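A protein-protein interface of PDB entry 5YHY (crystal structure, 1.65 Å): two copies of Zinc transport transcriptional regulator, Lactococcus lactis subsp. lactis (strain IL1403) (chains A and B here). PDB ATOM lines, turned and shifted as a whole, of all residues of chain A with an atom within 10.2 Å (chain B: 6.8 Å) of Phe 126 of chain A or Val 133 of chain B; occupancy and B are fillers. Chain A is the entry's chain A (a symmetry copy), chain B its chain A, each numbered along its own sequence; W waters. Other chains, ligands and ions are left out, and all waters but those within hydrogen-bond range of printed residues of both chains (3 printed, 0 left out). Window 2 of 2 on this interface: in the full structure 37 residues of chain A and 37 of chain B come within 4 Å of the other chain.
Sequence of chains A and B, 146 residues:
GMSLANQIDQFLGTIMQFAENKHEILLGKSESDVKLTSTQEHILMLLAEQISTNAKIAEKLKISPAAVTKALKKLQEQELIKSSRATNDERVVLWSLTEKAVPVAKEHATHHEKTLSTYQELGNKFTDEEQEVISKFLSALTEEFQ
OG of Ser 135 of chain B sits at hydrogen-bond distance from OE1 of Gln 7 of chain A, 2.6 Å away.
NE2 of Gln 131 of chain A lies within hydrogen-bond range of O of Gly 123 of chain A (2.9 Å).
O of Phe 126 of chain A is in hydrogen-bond range of NE2 of Gln 131 of chain A.
OE1 of Glu 130 of chain A is in hydrogen-bond range of N of Thr 127 of chain A, at 2.9 Å.
Among the printed residues, merely in contact across the chains: Leu 4 of chain A with Gln 131 of chain B (3.9 Å), Leu 122 of chain A with Phe 137 of chain B (3.9 Å), Leu 122 of chain A with Ala 140 of chain B (3.4 Å), Phe 126 of chain A with Val 133 of chain B (3.9 Å), Phe 126 of chain A with Phe 137 of chain B (3.7 Å), Glu 130 of chain A with Val 133 of chain B (3.8 Å), Gln 131 of chain A with Leu 4 of chain B (3.9 Å), Val 133 of chain A with Glu 130 of chain B (3.8 Å), Val 133 of chain A with Ile 134 of chain B (3.9 Å), Ile 134 of chain A with Val 133 of chain B (3.9 Å), Ile 134 of chain A with Phe 137 of chain B (3.8 Å) and Phe 137 of chain A with Ile 134 of chain B (3.8 Å).
Of chain A, only Phe 126, Glu 130 and Ile 134 come within 4 Å of Val 133 of chain B.
Of the printed residues of chain B, Leu 4 of chain A touches Gln 131.
Of the printed residues of chain A, Gln 131 of chain B touches Leu 4 (3.9 Å).
Printed residues of chain B within 4 Å of Val 133 of chain A: Glu 130 and Ile 134.
Of the printed residues of chain B, Ile 134 of chain A touches Val 133 and Phe 137.
Ser 135 of chain A touches none of the printed residues of chain B.
The nearest residue of chain B that does not touch Phe 126 of chain A is Lys 136 of chain B (4.3 Å).
The nearest residue of chain A that does not touch Val 133 of chain B is Val 133 of chain A (4.5 Å).
Hydrophobic or aromatic side chains of chain A that line the printed part of chain B: Leu 4, Leu 122, Phe 126, Val 133, Ile 134 and Phe 137.
Along chain A the printed residues that touch a printed residue of chain B span positions 4 to 137.
Among the printed residues, 13 pairs touch across the chains.
Among the printed residues, no Asp or Glu carboxylate lies within 4 Å of a Lys or Arg side-chain nitrogen of the other chain.
Leu 4 of chain A touches Gln 131 of chain B, and with the chains exchanged Gln 131 of chain A touches Leu 4 of chain B.
Glu 130 of chain A touches Val 133 of chain B, and with the chains exchanged Val 133 of chain A touches Glu 130 of chain B.
Val 133 of chain A touches Ile 134 of chain B, and with the chains exchanged Ile 134 of chain A touches Val 133 of chain B.
Ile 134 of chain A touches Phe 137 of chain B, and with the chains exchanged Phe 137 of chain A touches Ile 134 of chain B.
Water W3 lies within hydrogen-bond range of OE1 of Gln 120 of chain A (2.7 Å) and N of Leu 4 of chain B (3.3 Å).
Water W1 lies within hydrogen-bond range of the side-chain amide oxygen (OE1) of Gln 131 of chain B (3.0 Å) and the backbone NH (N) of Leu 4 of chain A (3.0 Å).
Water W2 bridges the side-chain amide oxygen (OE1) of Gln 131 of chain A (3.0 Å) and the backbone NH (N) of Leu 4 of chain B (3.0 Å).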
ATOM      1  N   LEU A   4     -10.966   3.499  21.495  1.00  0.00           N
ATOM      2  CA  LEU A   4     -10.819   3.362  20.052  1.00  0.00           C
ATOM      3  C   LEU A   4     -10.238   1.995  19.719  1.00  0.00           C
ATOM      4  O   LEU A   4     -10.634   1.377  18.735  1.00  0.00           O
ATOM      5  CB  LEU A   4      -9.952   4.471  19.456  1.00  0.00           C
ATOM      6  CG  LEU A   4      -9.841   4.472  17.926  1.00  0.00           C
ATOM      7  CD1 LEU A   4     -11.188   4.760  17.257  1.00  0.00           C
ATOM      8  CD2 LEU A   4      -8.789   5.463  17.444  1.00  0.00           C
ATOM      9  N   GLN A   7     -12.988  -0.364  19.674  1.00  0.00           N
ATOM     10  CA  GLN A   7     -13.829  -0.095  18.505  1.00  0.00           C
ATOM     11  C   GLN A   7     -13.201  -0.690  17.251  1.00  0.00           C
ATOM     12  O   GLN A   7     -13.897  -1.245  16.384  1.00  0.00           O
ATOM     13  CB  GLN A   7     -13.992   1.407  18.284  1.00  0.00           C
ATOM     14  CG  GLN A   7     -14.698   2.174  19.381  1.00  0.00           C
ATOM     15  CD  GLN A   7     -14.846   3.628  19.011  1.00  0.00           C
ATOM     16  OE1 GLN A   7     -15.050   3.960  17.831  1.00  0.00           O
ATOM     17  NE2 GLN A   7     -14.695   4.514  20.003  1.00  0.00           N
ATOM     18  N   THR A 118     -21.254   3.464  -2.250  1.00  0.00           N
ATOM     19  CA  THR A 118     -21.521   3.457  -0.819  1.00  0.00           C
ATOM     20  C   THR A 118     -20.352   4.065  -0.042  1.00  0.00           C
ATOM     21  O   THR A 118     -20.548   4.870   0.878  1.00  0.00           O
ATOM     22  CB  THR A 118     -21.813   2.028  -0.313  1.00  0.00           C
ATOM     23  OG1 THR A 118     -22.985   1.520  -0.968  1.00  0.00           O
ATOM     24  CG2 THR A 118     -22.032   2.017   1.203  1.00  0.00           C
ATOM     25  N   TYR A 119     -19.133   3.688  -0.410  1.00  0.00           N
ATOM     26  CA  TYR A 119     -17.958   4.247   0.257  1.00  0.00           C
ATOM     27  C   TYR A 119     -17.830   5.727  -0.077  1.00  0.00           C
ATOM     28  O   TYR A 119     -17.444   6.533   0.771  1.00  0.00           O
ATOM     29  CB  TYR A 119     -16.664   3.507  -0.125  1.00  0.00           C
ATOM     30  CG  TYR A 119     -16.676   2.016   0.163  1.00  0.00           C
ATOM     31  CD1 TYR A 119     -17.474   1.483   1.170  1.00  0.00           C
ATOM     32  CD2 TYR A 119     -15.889   1.144  -0.581  1.00  0.00           C
ATOM     33  CE1 TYR A 119     -17.492   0.113   1.412  1.00  0.00           C
ATOM     34  CE2 TYR A 119     -15.896  -0.217  -0.342  1.00  0.00           C
ATOM     35  CZ  TYR A 119     -16.699  -0.724   0.654  1.00  0.00           C
ATOM     36  OH  TYR A 119     -16.732  -2.073   0.898  1.00  0.00           O
ATOM     37  N   GLN A 120     -18.135   6.079  -1.322  1.00  0.00           N
ATOM     38  CA  GLN A 120     -18.042   7.471  -1.744  1.00  0.00           C
ATOM     39  C   GLN A 120     -19.009   8.348  -0.949  1.00  0.00           C
ATOM     40  O   GLN A 120     -18.629   9.413  -0.454  1.00  0.00           O
ATOM     41  CB  GLN A 120     -18.320   7.595  -3.242  1.00  0.00           C
ATOM     42  CG  GLN A 120     -18.209   9.005  -3.769  1.00  0.00           C
ATOM     43  CD  GLN A 120     -16.782   9.487  -3.811  1.00  0.00           C
ATOM     44  OE1 GLN A 120     -15.867   8.719  -4.104  1.00  0.00           O
ATOM     45  NE2 GLN A 120     -16.577  10.768  -3.518  1.00  0.00           N
ATOM     46  N   GLU A 121     -20.254   7.899  -0.825  1.00  0.00           N
ATOM     47  CA  GLU A 121     -21.254   8.651  -0.082  1.00  0.00           C
ATOM     48  C   GLU A 121     -20.847   8.811   1.373  1.00  0.00           C
ATOM     49  O   GLU A 121     -21.050   9.868   1.966  1.00  0.00           O
ATOM     50  CB  GLU A 121     -22.626   7.988  -0.185  1.00  0.00           C
ATOM     51  CG  GLU A 121     -23.211   8.063  -1.582  1.00  0.00           C
ATOM     52  CD  GLU A 121     -24.369   7.105  -1.784  1.00  0.00           C
ATOM     53  OE1 GLU A 121     -24.642   6.284  -0.878  1.00  0.00           O
ATOM     54  OE2 GLU A 121     -24.996   7.167  -2.865  1.00  0.00           O
ATOM     55  N   LEU A 122     -20.257   7.769   1.948  1.00  0.00           N
ATOM     56  CA  LEU A 122     -19.795   7.878   3.329  1.00  0.00           C
ATOM     57  C   LEU A 122     -18.662   8.907   3.430  1.00  0.00           C
ATOM     58  O   LEU A 122     -18.668   9.781   4.308  1.00  0.00           O
ATOM     59  CB  LEU A 122     -19.353   6.508   3.869  1.00  0.00           C
ATOM     60  CG  LEU A 122     -18.647   6.524   5.235  1.00  0.00           C
ATOM     61  CD1 LEU A 122     -19.471   7.269   6.276  1.00  0.00           C
ATOM     62  CD2 LEU A 122     -18.364   5.109   5.704  1.00  0.00           C
ATOM     63  N   GLY A 123     -17.686   8.800   2.535  1.00  0.00           N
ATOM     64  CA  GLY A 123     -16.570   9.730   2.527  1.00  0.00           C
ATOM     65  C   GLY A 123     -17.058  11.158   2.346  1.00  0.00           C
ATOM     66  O   GLY A 123     -16.513  12.080   2.961  1.00  0.00           O
ATOM     67  N   ASN A 124     -18.091  11.338   1.521  1.00  0.00           N
ATOM     68  CA  ASN A 124     -18.638  12.674   1.239  1.00  0.00           C
ATOM     69  C   ASN A 124     -19.175  13.381   2.473  1.00  0.00           C
ATOM     70  O   ASN A 124     -19.415  14.592   2.445  1.00  0.00           O
ATOM     71  CB  ASN A 124     -19.767  12.611   0.200  1.00  0.00           C
ATOM     72  CG  ASN A 124     -19.267  12.342  -1.207  1.00  0.00           C
ATOM     73  OD1 ASN A 124     -18.073  12.451  -1.498  1.00  0.00           O
ATOM     74  ND2 ASN A 124     -20.195  11.996  -2.099  1.00  0.00           N
ATOM     75  N   LYS A 125     -19.392  12.636   3.552  1.00  0.00           N
ATOM     76  CA  LYS A 125     -19.876  13.234   4.793  1.00  0.00           C
ATOM     77  C   LYS A 125     -18.751  13.889   5.582  1.00  0.00           C
ATOM     78  O   LYS A 125     -18.998  14.566   6.590  1.00  0.00           O
ATOM     79  CB  LYS A 125     -20.578  12.184   5.657  1.00  0.00           C
ATOM     80  CG  LYS A 125     -21.818  11.616   4.978  1.00  0.00           C
ATOM     81  CD  LYS A 125     -22.501  10.571   5.827  1.00  0.00           C
ATOM     82  CE  LYS A 125     -23.707   9.996   5.099  1.00  0.00           C
ATOM     83  NZ  LYS A 125     -24.260   8.810   5.830  1.00  0.00           N
ATOM     84  N   PHE A 126     -17.521  13.676   5.128  1.00  0.00           N
ATOM     85  CA  PHE A 126     -16.338  14.213   5.778  1.00  0.00           C
ATOM     86  C   PHE A 126     -15.639  15.257   4.900  1.00  0.00           C
ATOM     87  O   PHE A 126     -15.578  15.133   3.667  1.00  0.00           O
ATOM     88  CB  PHE A 126     -15.360  13.075   6.089  1.00  0.00           C
ATOM     89  CG  PHE A 126     -15.898  12.059   7.064  1.00  0.00           C
ATOM     90  CD1 PHE A 126     -15.707  12.228   8.432  1.00  0.00           C
ATOM     91  CD2 PHE A 126     -16.589  10.938   6.620  1.00  0.00           C
ATOM     92  CE1 PHE A 126     -16.190  11.294   9.332  1.00  0.00           C
ATOM     93  CE2 PHE A 126     -17.069   9.994   7.513  1.00  0.00           C
ATOM     94  CZ  PHE A 126     -16.882  10.177   8.869  1.00  0.00           C
ATOM     95  N   THR A 127     -15.120  16.293   5.544  1.00  0.00           N
ATOM     96  CA  THR A 127     -14.344  17.294   4.835  1.00  0.00           C
ATOM     97  C   THR A 127     -13.010  16.707   4.420  1.00  0.00           C
ATOM     98  O   THR A 127     -12.620  15.638   4.883  1.00  0.00           O
ATOM     99  CB  THR A 127     -14.036  18.494   5.735  1.00  0.00           C
ATOM    100  OG1 THR A 127     -13.201  18.068   6.825  1.00  0.00           O
ATOM    101  CG2 THR A 127     -15.327  19.099   6.268  1.00  0.00           C
ATOM    102  N   ASP A 128     -12.290  17.413   3.553  1.00  0.00           N
ATOM    103  CA  ASP A 128     -10.976  16.946   3.134  1.00  0.00           C
ATOM    104  C   ASP A 128     -10.032  16.725   4.311  1.00  0.00           C
ATOM    105  O   ASP A 128      -9.303  15.727   4.350  1.00  0.00           O
ATOM    106  CB  ASP A 128     -10.337  17.918   2.129  1.00  0.00           C
ATOM    107  CG  ASP A 128     -11.042  17.923   0.791  1.00  0.00           C
ATOM    108  OD1 ASP A 128     -11.454  16.844   0.308  1.00  0.00           O
ATOM    109  OD2 ASP A 128     -11.179  19.014   0.204  1.00  0.00           O
ATOM    110  N   GLU A 129     -10.032  17.658   5.266  1.00  0.00           N
ATOM    111  CA  GLU A 129      -9.173  17.544   6.437  1.00  0.00           C
ATOM    112  C   GLU A 129      -9.488  16.260   7.202  1.00  0.00           C
ATOM    113  O   GLU A 129      -8.578  15.546   7.630  1.00  0.00           O
ATOM    114  CB  GLU A 129      -9.349  18.756   7.355  1.00  0.00           C
ATOM    115  CG  GLU A 129      -8.714  18.596   8.733  1.00  0.00           C
ATOM    116  CD  GLU A 129      -8.845  19.839   9.604  1.00  0.00           C
ATOM    117  OE1 GLU A 129      -9.978  20.340   9.777  1.00  0.00           O
ATOM    118  OE2 GLU A 129      -7.806  20.313  10.120  1.00  0.00           O
ATOM    119  N   GLU A 130     -10.774  15.976   7.365  1.00  0.00           N
ATOM    120  CA  GLU A 130     -11.205  14.760   8.069  1.00  0.00           C
ATOM    121  C   GLU A 130     -10.862  13.522   7.253  1.00  0.00           C
ATOM    122  O   GLU A 130     -10.457  12.499   7.813  1.00  0.00           O
ATOM    123  CB  GLU A 130     -12.710  14.811   8.365  1.00  0.00           C
ATOM    124  CG  GLU A 130     -13.086  15.918   9.369  1.00  0.00           C
ATOM    125  CD  GLU A 130     -14.558  16.249   9.369  1.00  0.00           C
ATOM    126  OE1 GLU A 130     -15.275  15.841   8.435  1.00  0.00           O
ATOM    127  OE2 GLU A 130     -15.003  16.915  10.324  1.00  0.00           O
ATOM    128  N   GLN A 131     -11.025  13.598   5.936  1.00  0.00           N
ATOM    129  CA  GLN A 131     -10.649  12.471   5.084  1.00  0.00           C
ATOM    130  C   GLN A 131      -9.157  12.162   5.175  1.00  0.00           C
ATOM    131  O   GLN A 131      -8.760  11.006   5.104  1.00  0.00           O
ATOM    132  CB  GLN A 131     -11.052  12.693   3.627  1.00  0.00           C
ATOM    133  CG  GLN A 131     -12.540  12.747   3.410  1.00  0.00           C
ATOM    134  CD  GLN A 131     -12.880  12.785   1.936  1.00  0.00           C
ATOM    135  OE1 GLN A 131     -12.016  12.571   1.089  1.00  0.00           O
ATOM    136  NE2 GLN A 131     -14.128  13.083   1.621  1.00  0.00           N
ATOM    137  N   GLU A 132      -8.332  13.197   5.327  1.00  0.00           N
ATOM    138  CA  GLU A 132      -6.901  12.980   5.515  1.00  0.00           C
ATOM    139  C   GLU A 132      -6.618  12.180   6.791  1.00  0.00           C
ATOM    140  O   GLU A 132      -5.764  11.284   6.785  1.00  0.00           O
ATOM    141  CB  GLU A 132      -6.156  14.313   5.558  1.00  0.00           C
ATOM    142  CG  GLU A 132      -4.649  14.144   5.578  1.00  0.00           C
ATOM    143  CD  GLU A 132      -3.914  15.469   5.462  1.00  0.00           C
ATOM    144  OE1 GLU A 132      -4.492  16.514   5.847  1.00  0.00           O
ATOM    145  OE2 GLU A 132      -2.758  15.466   4.980  1.00  0.00           O
ATOM    146  N   VAL A 133      -7.330  12.503   7.873  1.00  0.00           N
ATOM    147  CA  VAL A 133      -7.184  11.764   9.126  1.00  0.00           C
ATOM    148  C   VAL A 133      -7.560  10.296   8.902  1.00  0.00           C
ATOM    149  O   VAL A 133      -6.815   9.387   9.271  1.00  0.00           O
ATOM    150  CB  VAL A 133      -8.061  12.356  10.251  1.00  0.00           C
ATOM    151  CG1 VAL A 133      -8.053  11.453  11.476  1.00  0.00           C
ATOM    152  CG2 VAL A 133      -7.566  13.758  10.615  1.00  0.00           C
ATOM    153  N   ILE A 134      -8.724  10.078   8.301  1.00  0.00           N
ATOM    154  CA  ILE A 134      -9.180   8.722   8.009  1.00  0.00           C
ATOM    155  C   ILE A 134      -8.165   7.983   7.135  1.00  0.00           C
ATOM    156  O   ILE A 134      -7.829   6.829   7.388  1.00  0.00           O
ATOM    157  CB  ILE A 134     -10.554   8.733   7.333  1.00  0.00           C
ATOM    158  CG1 ILE A 134     -11.598   9.314   8.288  1.00  0.00           C
ATOM    159  CG2 ILE A 134     -10.954   7.311   6.911  1.00  0.00           C
ATOM    160  CD1 ILE A 134     -12.909   9.731   7.596  1.00  0.00           C
ATOM    161  N   SER A 135      -7.674   8.656   6.101  1.00  0.00           N
ATOM    162  CA  SER A 135      -6.713   8.037   5.188  1.00  0.00           C
ATOM    163  C   SER A 135      -5.421   7.621   5.896  1.00  0.00           C
ATOM    164  O   SER A 135      -4.912   6.511   5.680  1.00  0.00           O
ATOM    165  CB  SER A 135      -6.402   8.995   4.031  1.00  0.00           C
ATOM    166  OG  SER A 135      -5.470   8.431   3.129  1.00  0.00           O
ATOM    167  N   LYS A 136      -4.893   8.506   6.738  1.00  0.00           N
ATOM    168  CA  LYS A 136      -3.690   8.201   7.510  1.00  0.00           C
ATOM    169  C   LYS A 136      -3.929   7.008   8.423  1.00  0.00           C
ATOM    170  O   LYS A 136      -3.082   6.121   8.519  1.00  0.00           O
ATOM    171  CB  LYS A 136      -3.231   9.424   8.313  1.00  0.00           C
ATOM    172  CG  LYS A 136      -2.651  10.506   7.412  1.00  0.00           C
ATOM    173  CD  LYS A 136      -2.149  11.705   8.205  1.00  0.00           C
ATOM    174  CE  LYS A 136      -0.835  11.401   8.898  1.00  0.00           C
ATOM    175  NZ  LYS A 136      -0.244  12.635   9.500  1.00  0.00           N
ATOM    176  N   PHE A 137      -5.098   6.989   9.057  1.00  0.00           N
ATOM    177  CA  PHE A 137      -5.502   5.869   9.892  1.00  0.00           C
ATOM    178  C   PHE A 137      -5.535   4.552   9.097  1.00  0.00           C
ATOM    179  O   PHE A 137      -4.965   3.537   9.520  1.00  0.00           O
ATOM    180  CB  PHE A 137      -6.877   6.142  10.522  1.00  0.00           C
ATOM    181  CG  PHE A 137      -7.427   4.962  11.262  1.00  0.00           C
ATOM    182  CD1 PHE A 137      -6.916   4.621  12.508  1.00  0.00           C
ATOM    183  CD2 PHE A 137      -8.436   4.194  10.712  1.00  0.00           C
ATOM    184  CE1 PHE A 137      -7.400   3.528  13.185  1.00  0.00           C
ATOM    185  CE2 PHE A 137      -8.927   3.089  11.395  1.00  0.00           C
ATOM    186  CZ  PHE A 137      -8.401   2.765  12.627  1.00  0.00           C
ATOM    187  N   LEU A 138      -6.213   4.562   7.958  1.00  0.00           N
ATOM    188  CA  LEU A 138      -6.335   3.345   7.167  1.00  0.00           C
ATOM    189  C   LEU A 138      -4.985   2.856   6.675  1.00  0.00           C
ATOM    190  O   LEU A 138      -4.731   1.653   6.651  1.00  0.00           O
ATOM    191  CB  LEU A 138      -7.276   3.543   5.984  1.00  0.00           C
ATOM    192  CG  LEU A 138      -8.734   3.766   6.373  1.00  0.00           C
ATOM    193  CD1 LEU A 138      -9.524   4.008   5.098  1.00  0.00           C
ATOM    194  CD2 LEU A 138      -9.270   2.568   7.143  1.00  0.00           C
ATOM    195  N   LEU B   4     -10.712   8.305  -1.499  1.00  0.00           N
ATOM    196  CA  LEU B   4     -10.936   7.633  -0.226  1.00  0.00           C
ATOM    197  C   LEU B   4     -11.770   6.378  -0.444  1.00  0.00           C
ATOM    198  O   LEU B   4     -11.531   5.357   0.196  1.00  0.00           O
ATOM    199  CB  LEU B   4     -11.608   8.550   0.796  1.00  0.00           C
ATOM    200  CG  LEU B   4     -11.776   7.961   2.202  1.00  0.00           C
ATOM    201  CD1 LEU B   4     -10.426   7.707   2.879  1.00  0.00           C
ATOM    202  CD2 LEU B   4     -12.647   8.852   3.079  1.00  0.00           C
ATOM    203  N   ASP B 128      -7.557  13.410  20.438  1.00  0.00           N
ATOM    204  CA  ASP B 128      -8.950  13.064  20.686  1.00  0.00           C
ATOM    205  C   ASP B 128      -9.872  13.508  19.556  1.00  0.00           C
ATOM    206  O   ASP B 128     -10.769  12.759  19.150  1.00  0.00           O
ATOM    207  CB  ASP B 128      -9.438  13.654  22.019  1.00  0.00           C
ATOM    208  CG  ASP B 128      -8.797  12.996  23.220  1.00  0.00           C
ATOM    209  OD1 ASP B 128      -8.607  11.758  23.216  1.00  0.00           O
ATOM    210  OD2 ASP B 128      -8.485  13.716  24.188  1.00  0.00           O
ATOM    211  N   GLU B 129      -9.665  14.727  19.053  1.00  0.00           N
ATOM    212  CA  GLU B 129     -10.485  15.248  17.967  1.00  0.00           C
ATOM    213  C   GLU B 129     -10.381  14.342  16.742  1.00  0.00           C
ATOM    214  O   GLU B 129     -11.389  14.037  16.100  1.00  0.00           O
ATOM    215  CB  GLU B 129     -10.056  16.672  17.603  1.00  0.00           C
ATOM    216  CG  GLU B 129     -10.656  17.193  16.301  1.00  0.00           C
ATOM    217  CD  GLU B 129     -10.266  18.633  15.994  1.00  0.00           C
ATOM    218  OE1 GLU B 129      -9.055  18.946  15.992  1.00  0.00           O
ATOM    219  OE2 GLU B 129     -11.181  19.455  15.750  1.00  0.00           O
ATOM    220  N   GLU B 130      -9.163  13.917  16.431  1.00  0.00           N
ATOM    221  CA  GLU B 130      -8.935  13.026  15.284  1.00  0.00           C
ATOM    222  C   GLU B 130      -9.530  11.650  15.551  1.00  0.00           C
ATOM    223  O   GLU B 130     -10.092  11.029  14.646  1.00  0.00           O
ATOM    224  CB  GLU B 130      -7.436  12.915  14.975  1.00  0.00           C
ATOM    225  CG  GLU B 130      -6.825  14.241  14.483  1.00  0.00           C
ATOM    226  CD  GLU B 130      -5.319  14.270  14.558  1.00  0.00           C
ATOM    227  OE1 GLU B 130      -4.725  13.400  15.224  1.00  0.00           O
ATOM    228  OE2 GLU B 130      -4.723  15.168  13.932  1.00  0.00           O
ATOM    229  N   GLN B 131      -9.405  11.164  16.782  1.00  0.00           N
ATOM    230  CA  GLN B 131     -10.013   9.880  17.128  1.00  0.00           C
ATOM    231  C   GLN B 131     -11.532   9.911  16.978  1.00  0.00           C
ATOM    232  O   GLN B 131     -12.136   8.916  16.598  1.00  0.00           O
ATOM    233  CB  GLN B 131      -9.633   9.425  18.536  1.00  0.00           C
ATOM    234  CG  GLN B 131      -8.170   9.115  18.699  1.00  0.00           C
ATOM    235  CD  GLN B 131      -7.885   8.499  20.052  1.00  0.00           C
ATOM    236  OE1 GLN B 131      -8.805   8.127  20.776  1.00  0.00           O
ATOM    237  NE2 GLN B 131      -6.616   8.414  20.411  1.00  0.00           N
ATOM    238  N   GLU B 132     -12.147  11.053  17.283  1.00  0.00           N
ATOM    239  CA  GLU B 132     -13.586  11.194  17.079  1.00  0.00           C
ATOM    240  C   GLU B 132     -13.961  11.035  15.602  1.00  0.00           C
ATOM    241  O   GLU B 132     -14.964  10.384  15.284  1.00  0.00           O
ATOM    242  CB  GLU B 132     -14.073  12.545  17.601  1.00  0.00           C
ATOM    243  CG  GLU B 132     -15.584  12.677  17.573  1.00  0.00           C
ATOM    244  CD  GLU B 132     -16.068  13.955  18.235  1.00  0.00           C
ATOM    245  OE1 GLU B 132     -15.295  14.942  18.277  1.00  0.00           O
ATOM    246  OE2 GLU B 132     -17.223  13.971  18.720  1.00  0.00           O
ATOM    247  N   VAL B 133     -13.161  11.627  14.712  1.00  0.00           N
ATOM    248  CA  VAL B 133     -13.391  11.489  13.275  1.00  0.00           C
ATOM    249  C   VAL B 133     -13.299  10.013  12.880  1.00  0.00           C
ATOM    250  O   VAL B 133     -14.183   9.479  12.208  1.00  0.00           O
ATOM    251  CB  VAL B 133     -12.379  12.310  12.447  1.00  0.00           C
ATOM    252  CG1 VAL B 133     -12.504  11.989  10.964  1.00  0.00           C
ATOM    253  CG2 VAL B 133     -12.595  13.806  12.692  1.00  0.00           C
ATOM    254  N   ILE B 134     -12.218   9.365  13.299  1.00  0.00           N
ATOM    255  CA  ILE B 134     -12.029   7.946  13.009  1.00  0.00           C
ATOM    256  C   ILE B 134     -13.195   7.119  13.554  1.00  0.00           C
ATOM    257  O   ILE B 134     -13.727   6.244  12.874  1.00  0.00           O
ATOM    258  CB  ILE B 134     -10.704   7.435  13.580  1.00  0.00           C
ATOM    259  CG1 ILE B 134      -9.535   8.147  12.897  1.00  0.00           C
ATOM    260  CG2 ILE B 134     -10.587   5.916  13.384  1.00  0.00           C
ATOM    261  CD1 ILE B 134      -8.197   8.007  13.647  1.00  0.00           C
ATOM    262  N   SER B 135     -13.594   7.401  14.789  1.00  0.00           N
ATOM    263  CA  SER B 135     -14.686   6.656  15.415  1.00  0.00           C
ATOM    264  C   SER B 135     -16.005   6.801  14.650  1.00  0.00           C
ATOM    265  O   SER B 135     -16.716   5.810  14.425  1.00  0.00           O
ATOM    266  CB  SER B 135     -14.861   7.113  16.869  1.00  0.00           C
ATOM    267  OG  SER B 135     -15.914   6.416  17.507  1.00  0.00           O
ATOM    268  N   LYS B 136     -16.329   8.028  14.251  1.00  0.00           N
ATOM    269  CA  LYS B 136     -17.537   8.282  13.468  1.00  0.00           C
ATOM    270  C   LYS B 136     -17.485   7.530  12.148  1.00  0.00           C
ATOM    271  O   LYS B 136     -18.476   6.926  11.738  1.00  0.00           O
ATOM    272  CB  LYS B 136     -17.733   9.785  13.238  1.00  0.00           C
ATOM    273  CG  LYS B 136     -18.141  10.504  14.518  1.00  0.00           C
ATOM    274  CD  LYS B 136     -18.384  11.989  14.288  1.00  0.00           C
ATOM    275  CE  LYS B 136     -19.704  12.233  13.583  1.00  0.00           C
ATOM    276  NZ  LYS B 136     -20.037  13.690  13.546  1.00  0.00           N
ATOM    277  N   PHE B 137     -16.316   7.552  11.514  1.00  0.00           N
ATOM    278  CA  PHE B 137     -16.092   6.804  10.287  1.00  0.00           C
ATOM    279  C   PHE B 137     -16.330   5.299  10.488  1.00  0.00           C
ATOM    280  O   PHE B 137     -17.059   4.659   9.719  1.00  0.00           O
ATOM    281  CB  PHE B 137     -14.666   7.050   9.766  1.00  0.00           C
ATOM    282  CG  PHE B 137     -14.314   6.185   8.596  1.00  0.00           C
ATOM    283  CD1 PHE B 137     -14.830   6.469   7.338  1.00  0.00           C
ATOM    284  CD2 PHE B 137     -13.483   5.091   8.755  1.00  0.00           C
ATOM    285  CE1 PHE B 137     -14.528   5.668   6.264  1.00  0.00           C
ATOM    286  CE2 PHE B 137     -13.177   4.280   7.670  1.00  0.00           C
ATOM    287  CZ  PHE B 137     -13.705   4.577   6.432  1.00  0.00           C
ATOM    288  N   LEU B 138     -15.706   4.729  11.510  1.00  0.00           N
ATOM    289  CA  LEU B 138     -15.839   3.298  11.745  1.00  0.00           C
ATOM    290  C   LEU B 138     -17.274   2.909  12.052  1.00  0.00           C
ATOM    291  O   LEU B 138     -17.743   1.865  11.605  1.00  0.00           O
ATOM    292  CB  LEU B 138     -14.924   2.832  12.872  1.00  0.00           C
ATOM    293  CG  LEU B 138     -13.436   2.921  12.548  1.00  0.00           C
ATOM    294  CD1 LEU B 138     -12.664   2.486  13.783  1.00  0.00           C
ATOM    295  CD2 LEU B 138     -13.098   2.054  11.345  1.00  0.00           C
ATOM    296  N   ALA B 140     -20.029   4.412  11.092  1.00  0.00           N
ATOM    297  CA  ALA B 140     -20.835   4.520   9.883  1.00  0.00           C
ATOM    298  C   ALA B 140     -20.540   3.378   8.927  1.00  0.00           C
ATOM    299  O   ALA B 140     -21.454   2.801   8.329  1.00  0.00           O
ATOM    300  CB  ALA B 140     -20.592   5.855   9.198  1.00  0.00           C
HETATM  301  O   HOH W   1      -9.343   5.830  22.550  1.00  0.00           O
HETATM  302  O   HOH W   2     -11.839  11.117  -1.474  1.00  0.00           O
HETATM  303  O   HOH W   3     -13.879   8.900  -2.238  1.00  0.00           O
